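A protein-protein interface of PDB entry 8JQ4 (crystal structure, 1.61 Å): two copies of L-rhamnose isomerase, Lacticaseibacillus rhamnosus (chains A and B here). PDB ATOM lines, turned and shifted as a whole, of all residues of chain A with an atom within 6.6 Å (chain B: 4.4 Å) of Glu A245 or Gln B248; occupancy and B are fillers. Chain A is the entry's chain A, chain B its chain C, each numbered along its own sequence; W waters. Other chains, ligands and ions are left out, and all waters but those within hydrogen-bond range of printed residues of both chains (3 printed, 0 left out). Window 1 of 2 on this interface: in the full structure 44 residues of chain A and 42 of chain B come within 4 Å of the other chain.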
ATOM      1  N   ARG A 203      20.628 -14.585   8.434  1.00  0.00           N
ATOM      2  CA  ARG A 203      20.705 -15.556   9.556  1.00  0.00           C
ATOM      3  C   ARG A 203      22.168 -15.973   9.778  1.00  0.00           C
ATOM      4  O   ARG A 203      22.541 -16.158  10.948  1.00  0.00           O
ATOM      5  CB  ARG A 203      19.735 -16.712   9.306  1.00  0.00           C
ATOM      6  CG  ARG A 203      18.299 -16.318   9.628  1.00  0.00           C
ATOM      7  CD  ARG A 203      17.231 -17.225   9.065  1.00  0.00           C
ATOM      8  NE  ARG A 203      15.930 -16.730   9.505  1.00  0.00           N
ATOM      9  CZ  ARG A 203      14.760 -17.259   9.171  1.00  0.00           C
ATOM     10  NH1 ARG A 203      14.706 -18.298   8.358  1.00  0.00           N
ATOM     11  NH2 ARG A 203      13.644 -16.737   9.650  1.00  0.00           N
ATOM     12  N   GLY A 242      15.757 -13.530  13.394  1.00  0.00           N
ATOM     13  CA  GLY A 242      15.778 -14.407  14.581  1.00  0.00           C
ATOM     14  C   GLY A 242      14.476 -15.176  14.737  1.00  0.00           C
ATOM     15  O   GLY A 242      13.628 -14.754  15.548  1.00  0.00           O
ATOM     16  N   SER A 243      14.325 -16.282  14.005  1.00  0.00           N
ATOM     17  CA  SER A 243      13.135 -17.169  14.056  1.00  0.00           C
ATOM     18  C   SER A 243      13.212 -18.072  15.293  1.00  0.00           C
ATOM     19  O   SER A 243      14.308 -18.206  15.881  1.00  0.00           O
ATOM     20  CB  SER A 243      13.001 -17.975  12.790  1.00  0.00           C
ATOM     21  OG  SER A 243      14.007 -18.972  12.707  1.00  0.00           O
ATOM     22  N   HIS A 244      12.083 -18.664  15.684  1.00  0.00           N
ATOM     23  CA  HIS A 244      12.006 -19.647  16.795  1.00  0.00           C
ATOM     24  C   HIS A 244      12.966 -20.808  16.508  1.00  0.00           C
ATOM     25  O   HIS A 244      13.635 -21.267  17.454  1.00  0.00           O
ATOM     26  CB  HIS A 244      10.566 -20.125  16.994  1.00  0.00           C
ATOM     27  CG  HIS A 244       9.645 -19.027  17.401  1.00  0.00           C
ATOM     28  ND1 HIS A 244       9.938 -18.166  18.440  1.00  0.00           N
ATOM     29  CD2 HIS A 244       8.444 -18.646  16.914  1.00  0.00           C
ATOM     30  CE1 HIS A 244       8.945 -17.308  18.587  1.00  0.00           C
ATOM     31  NE2 HIS A 244       8.022 -17.574  17.652  1.00  0.00           N
ATOM     32  N   GLU A 245      12.992 -21.288  15.263  1.00  0.00           N
ATOM     33  CA  GLU A 245      13.845 -22.433  14.846  1.00  0.00           C
ATOM     34  C   GLU A 245      15.307 -22.012  14.991  1.00  0.00           C
ATOM     35  O   GLU A 245      16.097 -22.775  15.583  1.00  0.00           O
ATOM     36  CB  GLU A 245      13.551 -22.854  13.404  1.00  0.00           C
ATOM     37  CG  GLU A 245      12.273 -23.652  13.241  1.00  0.00           C
ATOM     38  CD  GLU A 245      11.015 -22.807  13.216  1.00  0.00           C
ATOM     39  OE1 GLU A 245      11.140 -21.569  13.079  1.00  0.00           O
ATOM     40  OE2 GLU A 245       9.915 -23.395  13.298  1.00  0.00           O
ATOM     41  N   PHE A 246      15.651 -20.820  14.507  1.00  0.00           N
ATOM     42  CA  PHE A 246      17.043 -20.308  14.570  1.00  0.00           C
ATOM     43  C   PHE A 246      17.502 -20.302  16.032  1.00  0.00           C
ATOM     44  O   PHE A 246      18.608 -20.789  16.325  1.00  0.00           O
ATOM     45  CB  PHE A 246      17.178 -18.923  13.938  1.00  0.00           C
ATOM     46  CG  PHE A 246      18.580 -18.371  14.018  1.00  0.00           C
ATOM     47  CD1 PHE A 246      19.504 -18.644  13.024  1.00  0.00           C
ATOM     48  CD2 PHE A 246      18.989 -17.638  15.118  1.00  0.00           C
ATOM     49  CE1 PHE A 246      20.809 -18.183  13.126  1.00  0.00           C
ATOM     50  CE2 PHE A 246      20.284 -17.156  15.207  1.00  0.00           C
ATOM     51  CZ  PHE A 246      21.188 -17.418  14.203  1.00  0.00           C
ATOM     52  N   TYR A 247      16.688 -19.768  16.945  1.00  0.00           N
ATOM     53  CA  TYR A 247      17.118 -19.523  18.345  1.00  0.00           C
ATOM     54  C   TYR A 247      17.068 -20.814  19.170  1.00  0.00           C
ATOM     55  O   TYR A 247      17.932 -20.966  20.048  1.00  0.00           O
ATOM     56  CB  TYR A 247      16.303 -18.414  19.003  1.00  0.00           C
ATOM     57  CG  TYR A 247      16.709 -17.018  18.603  1.00  0.00           C
ATOM     58  CD1 TYR A 247      18.020 -16.583  18.710  1.00  0.00           C
ATOM     59  CD2 TYR A 247      15.757 -16.110  18.170  1.00  0.00           C
ATOM     60  CE1 TYR A 247      18.377 -15.287  18.377  1.00  0.00           C
ATOM     61  CE2 TYR A 247      16.098 -14.811  17.838  1.00  0.00           C
ATOM     62  CZ  TYR A 247      17.410 -14.393  17.953  1.00  0.00           C
ATOM     63  OH  TYR A 247      17.733 -13.107  17.638  1.00  0.00           O
ATOM     64  N   GLN A 248      16.141 -21.736  18.899  1.00  0.00           N
ATOM     65  CA  GLN A 248      16.176 -23.051  19.584  1.00  0.00           C
ATOM     66  C   GLN A 248      17.490 -23.742  19.191  1.00  0.00           C
ATOM     67  O   GLN A 248      18.182 -24.247  20.094  1.00  0.00           O
ATOM     68  CB  GLN A 248      14.978 -23.951  19.280  1.00  0.00           C
ATOM     69  CG  GLN A 248      15.082 -25.262  20.050  1.00  0.00           C
ATOM     70  CD  GLN A 248      13.802 -26.042  20.219  1.00  0.00           C
ATOM     71  OE1 GLN A 248      13.760 -27.022  20.962  1.00  0.00           O
ATOM     72  NE2 GLN A 248      12.748 -25.615  19.537  1.00  0.00           N
ATOM     73  N   ASN A 249      17.827 -23.725  17.900  1.00  0.00           N
ATOM     74  CA  ASN A 249      19.071 -24.347  17.367  1.00  0.00           C
ATOM     75  C   ASN A 249      20.280 -23.659  18.006  1.00  0.00           C
ATOM     76  O   ASN A 249      21.250 -24.362  18.382  1.00  0.00           O
ATOM     77  CB  ASN A 249      19.142 -24.258  15.843  1.00  0.00           C
ATOM     78  CG  ASN A 249      18.154 -25.170  15.149  1.00  0.00           C
ATOM     79  OD1 ASN A 249      17.647 -26.115  15.753  1.00  0.00           O
ATOM     80  ND2 ASN A 249      17.916 -24.922  13.870  1.00  0.00           N
ATOM     81  N   TYR A 250      20.250 -22.328  18.085  1.00  0.00           N
ATOM     82  CA  TYR A 250      21.361 -21.511  18.632  1.00  0.00           C
ATOM     83  C   TYR A 250      21.541 -21.817  20.122  1.00  0.00           C
ATOM     84  O   TYR A 250      22.687 -22.059  20.551  1.00  0.00           O
ATOM     85  CB  TYR A 250      21.132 -20.015  18.416  1.00  0.00           C
ATOM     86  CG  TYR A 250      22.341 -19.197  18.781  1.00  0.00           C
ATOM     87  CD1 TYR A 250      23.428 -19.140  17.927  1.00  0.00           C
ATOM     88  CD2 TYR A 250      22.465 -18.618  20.032  1.00  0.00           C
ATOM     89  CE1 TYR A 250      24.582 -18.461  18.277  1.00  0.00           C
ATOM     90  CE2 TYR A 250      23.609 -17.929  20.396  1.00  0.00           C
ATOM     91  CZ  TYR A 250      24.677 -17.861  19.519  1.00  0.00           C
ATOM     92  OH  TYR A 250      25.808 -17.185  19.866  1.00  0.00           O
ATOM     93  N   TRP A 258      16.693 -20.632  25.901  1.00  0.00           N
ATOM     94  CA  TRP A 258      15.768 -20.307  24.790  1.00  0.00           C
ATOM     95  C   TRP A 258      14.536 -19.617  25.378  1.00  0.00           C
ATOM     96  O   TRP A 258      14.024 -20.122  26.397  1.00  0.00           O
ATOM     97  CB  TRP A 258      15.403 -21.578  24.017  1.00  0.00           C
ATOM     98  CG  TRP A 258      14.481 -21.338  22.864  1.00  0.00           C
ATOM     99  CD1 TRP A 258      14.508 -20.291  21.989  1.00  0.00           C
ATOM    100  CD2 TRP A 258      13.416 -22.197  22.428  1.00  0.00           C
ATOM    101  NE1 TRP A 258      13.511 -20.421  21.061  1.00  0.00           N
ATOM    102  CE2 TRP A 258      12.820 -21.578  21.310  1.00  0.00           C
ATOM    103  CE3 TRP A 258      12.882 -23.400  22.901  1.00  0.00           C
ATOM    104  CZ2 TRP A 258      11.716 -22.125  20.662  1.00  0.00           C
ATOM    105  CZ3 TRP A 258      11.806 -23.952  22.243  1.00  0.00           C
ATOM    106  CH2 TRP A 258      11.228 -23.316  21.145  1.00  0.00           C
ATOM    107  N   HIS A 266       2.344 -18.931  15.713  1.00  0.00           N
ATOM    108  CA  HIS A 266       1.304 -19.012  14.659  1.00  0.00           C
ATOM    109  C   HIS A 266      -0.071 -19.028  15.312  1.00  0.00           C
ATOM    110  O   HIS A 266      -0.226 -19.411  16.469  1.00  0.00           O
ATOM    111  CB  HIS A 266       1.487 -20.252  13.775  1.00  0.00           C
ATOM    112  CG  HIS A 266       2.692 -20.194  12.901  1.00  0.00           C
ATOM    113  ND1 HIS A 266       3.934 -20.602  13.343  1.00  0.00           N
ATOM    114  CD2 HIS A 266       2.860 -19.752  11.636  1.00  0.00           C
ATOM    115  CE1 HIS A 266       4.816 -20.420  12.384  1.00  0.00           C
ATOM    116  NE2 HIS A 266       4.186 -19.898  11.325  1.00  0.00           N
ATOM    117  N   GLU A 269      -1.124 -22.196  17.461  1.00  0.00           N
ATOM    118  CA  GLU A 269       0.138 -22.833  17.934  1.00  0.00           C
ATOM    119  C   GLU A 269       0.127 -22.876  19.467  1.00  0.00           C
ATOM    120  O   GLU A 269      -0.156 -21.833  20.094  1.00  0.00           O
ATOM    121  CB  GLU A 269       1.357 -22.094  17.385  1.00  0.00           C
ATOM    122  CG  GLU A 269       2.678 -22.786  17.698  1.00  0.00           C
ATOM    123  CD  GLU A 269       3.754 -22.525  16.660  1.00  0.00           C
ATOM    124  OE1 GLU A 269       4.706 -23.326  16.575  1.00  0.00           O
ATOM    125  OE2 GLU A 269       3.638 -21.516  15.942  1.00  0.00           O
ATOM    126  N   HIS B 244       7.934 -31.451  15.064  1.00  0.00           N
ATOM    127  CA  HIS B 244       8.923 -30.778  14.183  1.00  0.00           C
ATOM    128  C   HIS B 244      10.144 -30.357  15.012  1.00  0.00           C
ATOM    129  O   HIS B 244      11.278 -30.562  14.538  1.00  0.00           O
ATOM    130  CB  HIS B 244       8.277 -29.607  13.439  1.00  0.00           C
ATOM    131  CG  HIS B 244       7.157 -30.024  12.548  1.00  0.00           C
ATOM    132  ND1 HIS B 244       7.308 -30.994  11.571  1.00  0.00           N
ATOM    133  CD2 HIS B 244       5.875 -29.600  12.475  1.00  0.00           C
ATOM    134  CE1 HIS B 244       6.159 -31.160  10.945  1.00  0.00           C
ATOM    135  NE2 HIS B 244       5.259 -30.315  11.486  1.00  0.00           N
ATOM    136  N   GLU B 245       9.922 -29.778  16.193  1.00  0.00           N
ATOM    137  CA  GLU B 245      11.013 -29.305  17.088  1.00  0.00           C
ATOM    138  C   GLU B 245      11.856 -30.514  17.490  1.00  0.00           C
ATOM    139  O   GLU B 245      13.106 -30.431  17.394  1.00  0.00           O
ATOM    140  CB  GLU B 245      10.456 -28.606  18.331  1.00  0.00           C
ATOM    141  CG  GLU B 245       9.902 -27.220  18.053  1.00  0.00           C
ATOM    142  CD  GLU B 245       8.503 -27.176  17.455  1.00  0.00           C
ATOM    143  OE1 GLU B 245       8.097 -26.088  17.002  1.00  0.00           O
ATOM    144  OE2 GLU B 245       7.820 -28.223  17.449  1.00  0.00           O
ATOM    145  N   PHE B 246      11.204 -31.598  17.917  1.00  0.00           N
ATOM    146  CA  PHE B 246      11.901 -32.820  18.390  1.00  0.00           C
ATOM    147  C   PHE B 246      12.844 -33.303  17.283  1.00  0.00           C
ATOM    148  O   PHE B 246      14.030 -33.579  17.572  1.00  0.00           O
ATOM    149  CB  PHE B 246      10.935 -33.929  18.805  1.00  0.00           C
ATOM    150  CG  PHE B 246      11.648 -35.198  19.207  1.00  0.00           C
ATOM    151  CD1 PHE B 246      12.011 -35.422  20.524  1.00  0.00           C
ATOM    152  CD2 PHE B 246      12.021 -36.129  18.253  1.00  0.00           C
ATOM    153  CE1 PHE B 246      12.700 -36.569  20.882  1.00  0.00           C
ATOM    154  CE2 PHE B 246      12.720 -37.271  18.611  1.00  0.00           C
ATOM    155  CZ  PHE B 246      13.042 -37.496  19.927  1.00  0.00           C
ATOM    156  N   TYR B 247      12.342 -33.406  16.051  1.00  0.00           N
ATOM    157  CA  TYR B 247      13.085 -34.026  14.928  1.00  0.00           C
ATOM    158  C   TYR B 247      14.135 -33.057  14.380  1.00  0.00           C
ATOM    159  O   TYR B 247      15.211 -33.550  13.994  1.00  0.00           O
ATOM    160  CB  TYR B 247      12.156 -34.526  13.827  1.00  0.00           C
ATOM    161  CG  TYR B 247      11.459 -35.821  14.149  1.00  0.00           C
ATOM    162  CD1 TYR B 247      12.147 -36.922  14.635  1.00  0.00           C
ATOM    163  CD2 TYR B 247      10.102 -35.962  13.917  1.00  0.00           C
ATOM    164  CE1 TYR B 247      11.501 -38.118  14.903  1.00  0.00           C
ATOM    165  CE2 TYR B 247       9.445 -37.154  14.163  1.00  0.00           C
ATOM    166  CZ  TYR B 247      10.146 -38.239  14.656  1.00  0.00           C
ATOM    167  OH  TYR B 247       9.492 -39.413  14.895  1.00  0.00           O
ATOM    168  N   GLN B 248      13.877 -31.746  14.347  1.00  0.00           N
ATOM    169  CA  GLN B 248      14.939 -30.793  13.927  1.00  0.00           C
ATOM    170  C   GLN B 248      16.107 -30.914  14.918  1.00  0.00           C
ATOM    171  O   GLN B 248      17.274 -31.026  14.464  1.00  0.00           O
ATOM    172  CB  GLN B 248      14.457 -29.347  13.793  1.00  0.00           C
ATOM    173  CG  GLN B 248      15.596 -28.422  13.385  1.00  0.00           C
ATOM    174  CD  GLN B 248      15.227 -27.090  12.779  1.00  0.00           C
ATOM    175  OE1 GLN B 248      16.078 -26.404  12.216  1.00  0.00           O
ATOM    176  NE2 GLN B 248      13.974 -26.684  12.939  1.00  0.00           N
ATOM    177  N   ASN B 249      15.801 -30.960  16.219  1.00  0.00           N
ATOM    178  CA  ASN B 249      16.799 -31.117  17.310  1.00  0.00           C
ATOM    179  C   ASN B 249      17.516 -32.460  17.132  1.00  0.00           C
ATOM    180  O   ASN B 249      18.768 -32.505  17.280  1.00  0.00           O
ATOM    181  CB  ASN B 249      16.142 -31.011  18.687  1.00  0.00           C
ATOM    182  CG  ASN B 249      15.726 -29.601  19.047  1.00  0.00           C
ATOM    183  OD1 ASN B 249      16.183 -28.633  18.441  1.00  0.00           O
ATOM    184  ND2 ASN B 249      14.823 -29.482  20.012  1.00  0.00           N
ATOM    185  N   TYR B 250      16.760 -33.523  16.854  1.00  0.00           N
ATOM    186  CA  TYR B 250      17.300 -34.898  16.722  1.00  0.00           C
ATOM    187  C   TYR B 250      18.228 -34.963  15.505  1.00  0.00           C
ATOM    188  O   TYR B 250      19.369 -35.457  15.647  1.00  0.00           O
ATOM    189  CB  TYR B 250      16.193 -35.948  16.627  1.00  0.00           C
ATOM    190  CG  TYR B 250      16.730 -37.353  16.706  1.00  0.00           C
ATOM    191  CD1 TYR B 250      17.085 -37.908  17.924  1.00  0.00           C
ATOM    192  CD2 TYR B 250      16.990 -38.088  15.561  1.00  0.00           C
ATOM    193  CE1 TYR B 250      17.634 -39.177  18.008  1.00  0.00           C
ATOM    194  CE2 TYR B 250      17.551 -39.355  15.626  1.00  0.00           C
ATOM    195  CZ  TYR B 250      17.871 -39.900  16.855  1.00  0.00           C
ATOM    196  OH  TYR B 250      18.384 -41.162  16.938  1.00  0.00           O
ATOM    197  N   ALA B 251      17.777 -34.465  14.348  1.00  0.00           N
ATOM    198  CA  ALA B 251      18.570 -34.489  13.096  1.00  0.00           C
ATOM    199  C   ALA B 251      19.892 -33.747  13.319  1.00  0.00           C
ATOM    200  O   ALA B 251      20.951 -34.300  12.950  1.00  0.00           O
ATOM    201  CB  ALA B 251      17.800 -33.902  11.942  1.00  0.00           C
ATOM    202  N   ILE B 252      19.850 -32.544  13.897  1.00  0.00           N
ATOM    203  CA  ILE B 252      21.076 -31.717  14.112  1.00  0.00           C
ATOM    204  C   ILE B 252      22.002 -32.449  15.092  1.00  0.00           C
ATOM    205  O   ILE B 252      23.216 -32.569  14.786  1.00  0.00           O
ATOM    206  CB  ILE B 252      20.724 -30.295  14.585  1.00  0.00           C
ATOM    207  CG1 ILE B 252      20.038 -29.500  13.471  1.00  0.00           C
ATOM    208  CG2 ILE B 252      21.963 -29.585  15.110  1.00  0.00           C
ATOM    209  CD1 ILE B 252      19.443 -28.185  13.922  1.00  0.00           C
ATOM    210  N   TRP B 258      16.623 -33.914   8.208  1.00  0.00           N
ATOM    211  CA  TRP B 258      15.302 -33.498   8.736  1.00  0.00           C
ATOM    212  C   TRP B 258      14.297 -33.459   7.580  1.00  0.00           C
ATOM    213  O   TRP B 258      14.635 -32.889   6.529  1.00  0.00           O
ATOM    214  CB  TRP B 258      15.442 -32.148   9.440  1.00  0.00           C
ATOM    215  CG  TRP B 258      14.168 -31.652  10.046  1.00  0.00           C
ATOM    216  CD1 TRP B 258      13.220 -32.388  10.693  1.00  0.00           C
ATOM    217  CD2 TRP B 258      13.707 -30.292  10.061  1.00  0.00           C
ATOM    218  NE1 TRP B 258      12.196 -31.578  11.108  1.00  0.00           N
ATOM    219  CE2 TRP B 258      12.468 -30.290  10.732  1.00  0.00           C
ATOM    220  CE3 TRP B 258      14.217 -29.085   9.570  1.00  0.00           C
ATOM    221  CZ2 TRP B 258      11.735 -29.122  10.919  1.00  0.00           C
ATOM    222  CZ3 TRP B 258      13.499 -27.929   9.774  1.00  0.00           C
ATOM    223  CH2 TRP B 258      12.269 -27.953  10.429  1.00  0.00           C
ATOM    224  N   GLU B 269       1.430 -21.317   8.311  1.00  0.00           N
ATOM    225  CA  GLU B 269       2.886 -21.578   8.507  1.00  0.00           C
ATOM    226  C   GLU B 269       3.548 -21.741   7.133  1.00  0.00           C
ATOM    227  O   GLU B 269       3.007 -22.480   6.290  1.00  0.00           O
ATOM    228  CB  GLU B 269       3.121 -22.784   9.418  1.00  0.00           C
ATOM    229  CG  GLU B 269       4.570 -22.942   9.847  1.00  0.00           C
ATOM    230  CD  GLU B 269       4.729 -23.652  11.180  1.00  0.00           C
ATOM    231  OE1 GLU B 269       3.758 -24.306  11.614  1.00  0.00           O
ATOM    232  OE2 GLU B 269       5.812 -23.538  11.791  1.00  0.00           O
ATOM    233  N   LYS B 274      11.911 -22.213   7.037  1.00  0.00           N
ATOM    234  CA  LYS B 274      12.694 -23.113   7.937  1.00  0.00           C
ATOM    235  C   LYS B 274      14.116 -23.323   7.398  1.00  0.00           C
ATOM    236  O   LYS B 274      15.016 -23.511   8.228  1.00  0.00           O
ATOM    237  CB  LYS B 274      12.020 -24.476   8.114  1.00  0.00           C
ATOM    238  CG  LYS B 274      10.532 -24.435   8.442  1.00  0.00           C
ATOM    239  CD  LYS B 274      10.197 -23.718   9.723  1.00  0.00           C
ATOM    240  CE  LYS B 274       8.723 -23.810  10.057  1.00  0.00           C
ATOM    241  NZ  LYS B 274       8.353 -22.885  11.152  1.00  0.00           N
ATOM    242  N   ALA B 277      17.073 -21.295   8.634  1.00  0.00           N
ATOM    243  CA  ALA B 277      17.200 -21.403  10.106  1.00  0.00           C
ATOM    244  C   ALA B 277      17.809 -22.764  10.477  1.00  0.00           C
ATOM    245  O   ALA B 277      18.306 -22.903  11.606  1.00  0.00           O
ATOM    246  CB  ALA B 277      15.861 -21.188  10.768  1.00  0.00           C
ATOM    247  N   PHE B 278      17.779 -23.721   9.548  1.00  0.00           N
ATOM    248  CA  PHE B 278      18.306 -25.099   9.728  1.00  0.00           C
ATOM    249  C   PHE B 278      19.780 -25.146   9.307  1.00  0.00           C
ATOM    250  O   PHE B 278      20.607 -25.731  10.040  1.00  0.00           O
ATOM    251  CB  PHE B 278      17.477 -26.096   8.919  1.00  0.00           C
ATOM    252  CG  PHE B 278      18.042 -27.492   8.883  1.00  0.00           C
ATOM    253  CD1 PHE B 278      17.894 -28.345   9.964  1.00  0.00           C
ATOM    254  CD2 PHE B 278      18.732 -27.946   7.771  1.00  0.00           C
ATOM    255  CE1 PHE B 278      18.413 -29.631   9.929  1.00  0.00           C
ATOM    256  CE2 PHE B 278      19.250 -29.230   7.738  1.00  0.00           C
ATOM    257  CZ  PHE B 278      19.093 -30.067   8.817  1.00  0.00           C
HETATM  258  O   HOH W   1      18.679 -28.042  17.532  1.00  0.00           O
HETATM  259  O   HOH W   2      12.646 -25.931  16.064  1.00  0.00           O
HETATM  260  O   HOH W   3      15.129 -26.763  16.651  1.00  0.00           O
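The side-chain amino group (NZ) of Lys B274 lies within salt-bridge range of the side-chain carboxylate (OE2) of Glu A245 (2.7 Å).
The side-chain amide oxygen (OE1) of Gln A248 sits at hydrogen-bond distance from the side-chain amide nitrogen (ND2) of Asn B249 (2.8 Å).
The side-chain amide nitrogen of Asn A249 sits at hydrogen-bond distance from the side-chain amide oxygen of Gln B248, at 2.9 Å.
ND2 of Asn A249 sits at hydrogen-bond distance from O of Ala B277, 3.1 Å away.
OG of Ser A243 sits at hydrogen-bond distance from N of Phe A246 (3.1 Å).
The side-chain amide nitrogen (ND2) of Asn A249 lies close to the backbone carbonyl oxygen (O) of Glu A245 (3.3 Å).
A ring nitrogen (ND1) of His A266 lies within hydrogen-bond range of the side-chain carboxylate (OE2) of Glu A269, 2.8 Å away.
The side-chain amide nitrogen of Asn B249 lies close to the backbone carbonyl oxygen of Glu B245 (3.3 Å).
The side-chain carboxylate of Glu B269 is in salt-bridge range of the side-chain amino group of Lys B274, 2.7 Å away.
Among the printed residues, pairs that only touch across the chains: Arg A203 with Ala B277 (3.8 Å), Ser A243 with Ala B277 (3.5 Å), Glu A245 with Gln B248 (3.5 Å), Glu A245 with Ala B277 (3.9 Å), Phe A246 with Ala B277 (3.8 Å), Gln A248 with Glu B245 (3.6 Å), Asn A249 with Asn B249 (3.96 Å), Asn A249 with Ile B252 (3.3 Å) and His A266 with Glu B269 (3.3 Å).
Of the printed residues of chain A, Asn B249 touches Gln A248 and Asn A249.
Of the printed residues of chain B, Arg A203 touches Ala B277.
Tyr B250 touches none of the printed residues of chain A.
The nearest printed residue of chain B that does not touch Glu A245 is Glu B269 (4.4 Å).
The nearest residue of chain A that does not touch Gln B248 is Phe A246 (6.1 Å).
The nearest printed residue of chain B that does not touch Ser A243 is Lys B274 (6.5 Å).
Hydrophobic or aromatic side chains of chain A that line the printed part of chain B: His A266.
Of the 14 printed residues of chain B, 7 touch a printed residue of chain A.
Hydrophobic or aromatic side chains of chain B within 4 Å of the printed part of chain A: Ile B252 and Ala B277.
Among the printed residues, 13 pairs touch across the chains.
Among the printed residues, Asp or Glu carboxylates within 4 Å of a Lys or Arg side-chain nitrogen of the other chain: Glu A245 with Lys B274 (2.7 Å).
Glu A245 touches Gln B248, and with the chains exchanged Gln A248 touches Glu B245.
Gln A248 touches Asn B249, and with the chains exchanged Asn A249 touches Gln B248.
Asn B249 touches its own counterpart, Asn A249.
Water W1 bridges OD1 of Asn B249 (2.7 Å) and OD1 of Asn A249 (2.8 Å).
Water W3 bridges the side-chain amide oxygen of Asn A249 (2.8 Å) and the side-chain amide oxygen of Asn B249 (2.8 Å).
Water W2 lies within hydrogen-bond range of the side-chain amide nitrogen of Gln B248 (3.5 Å) and the side-chain amide nitrogen of Gln A248 (3.5 Å).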
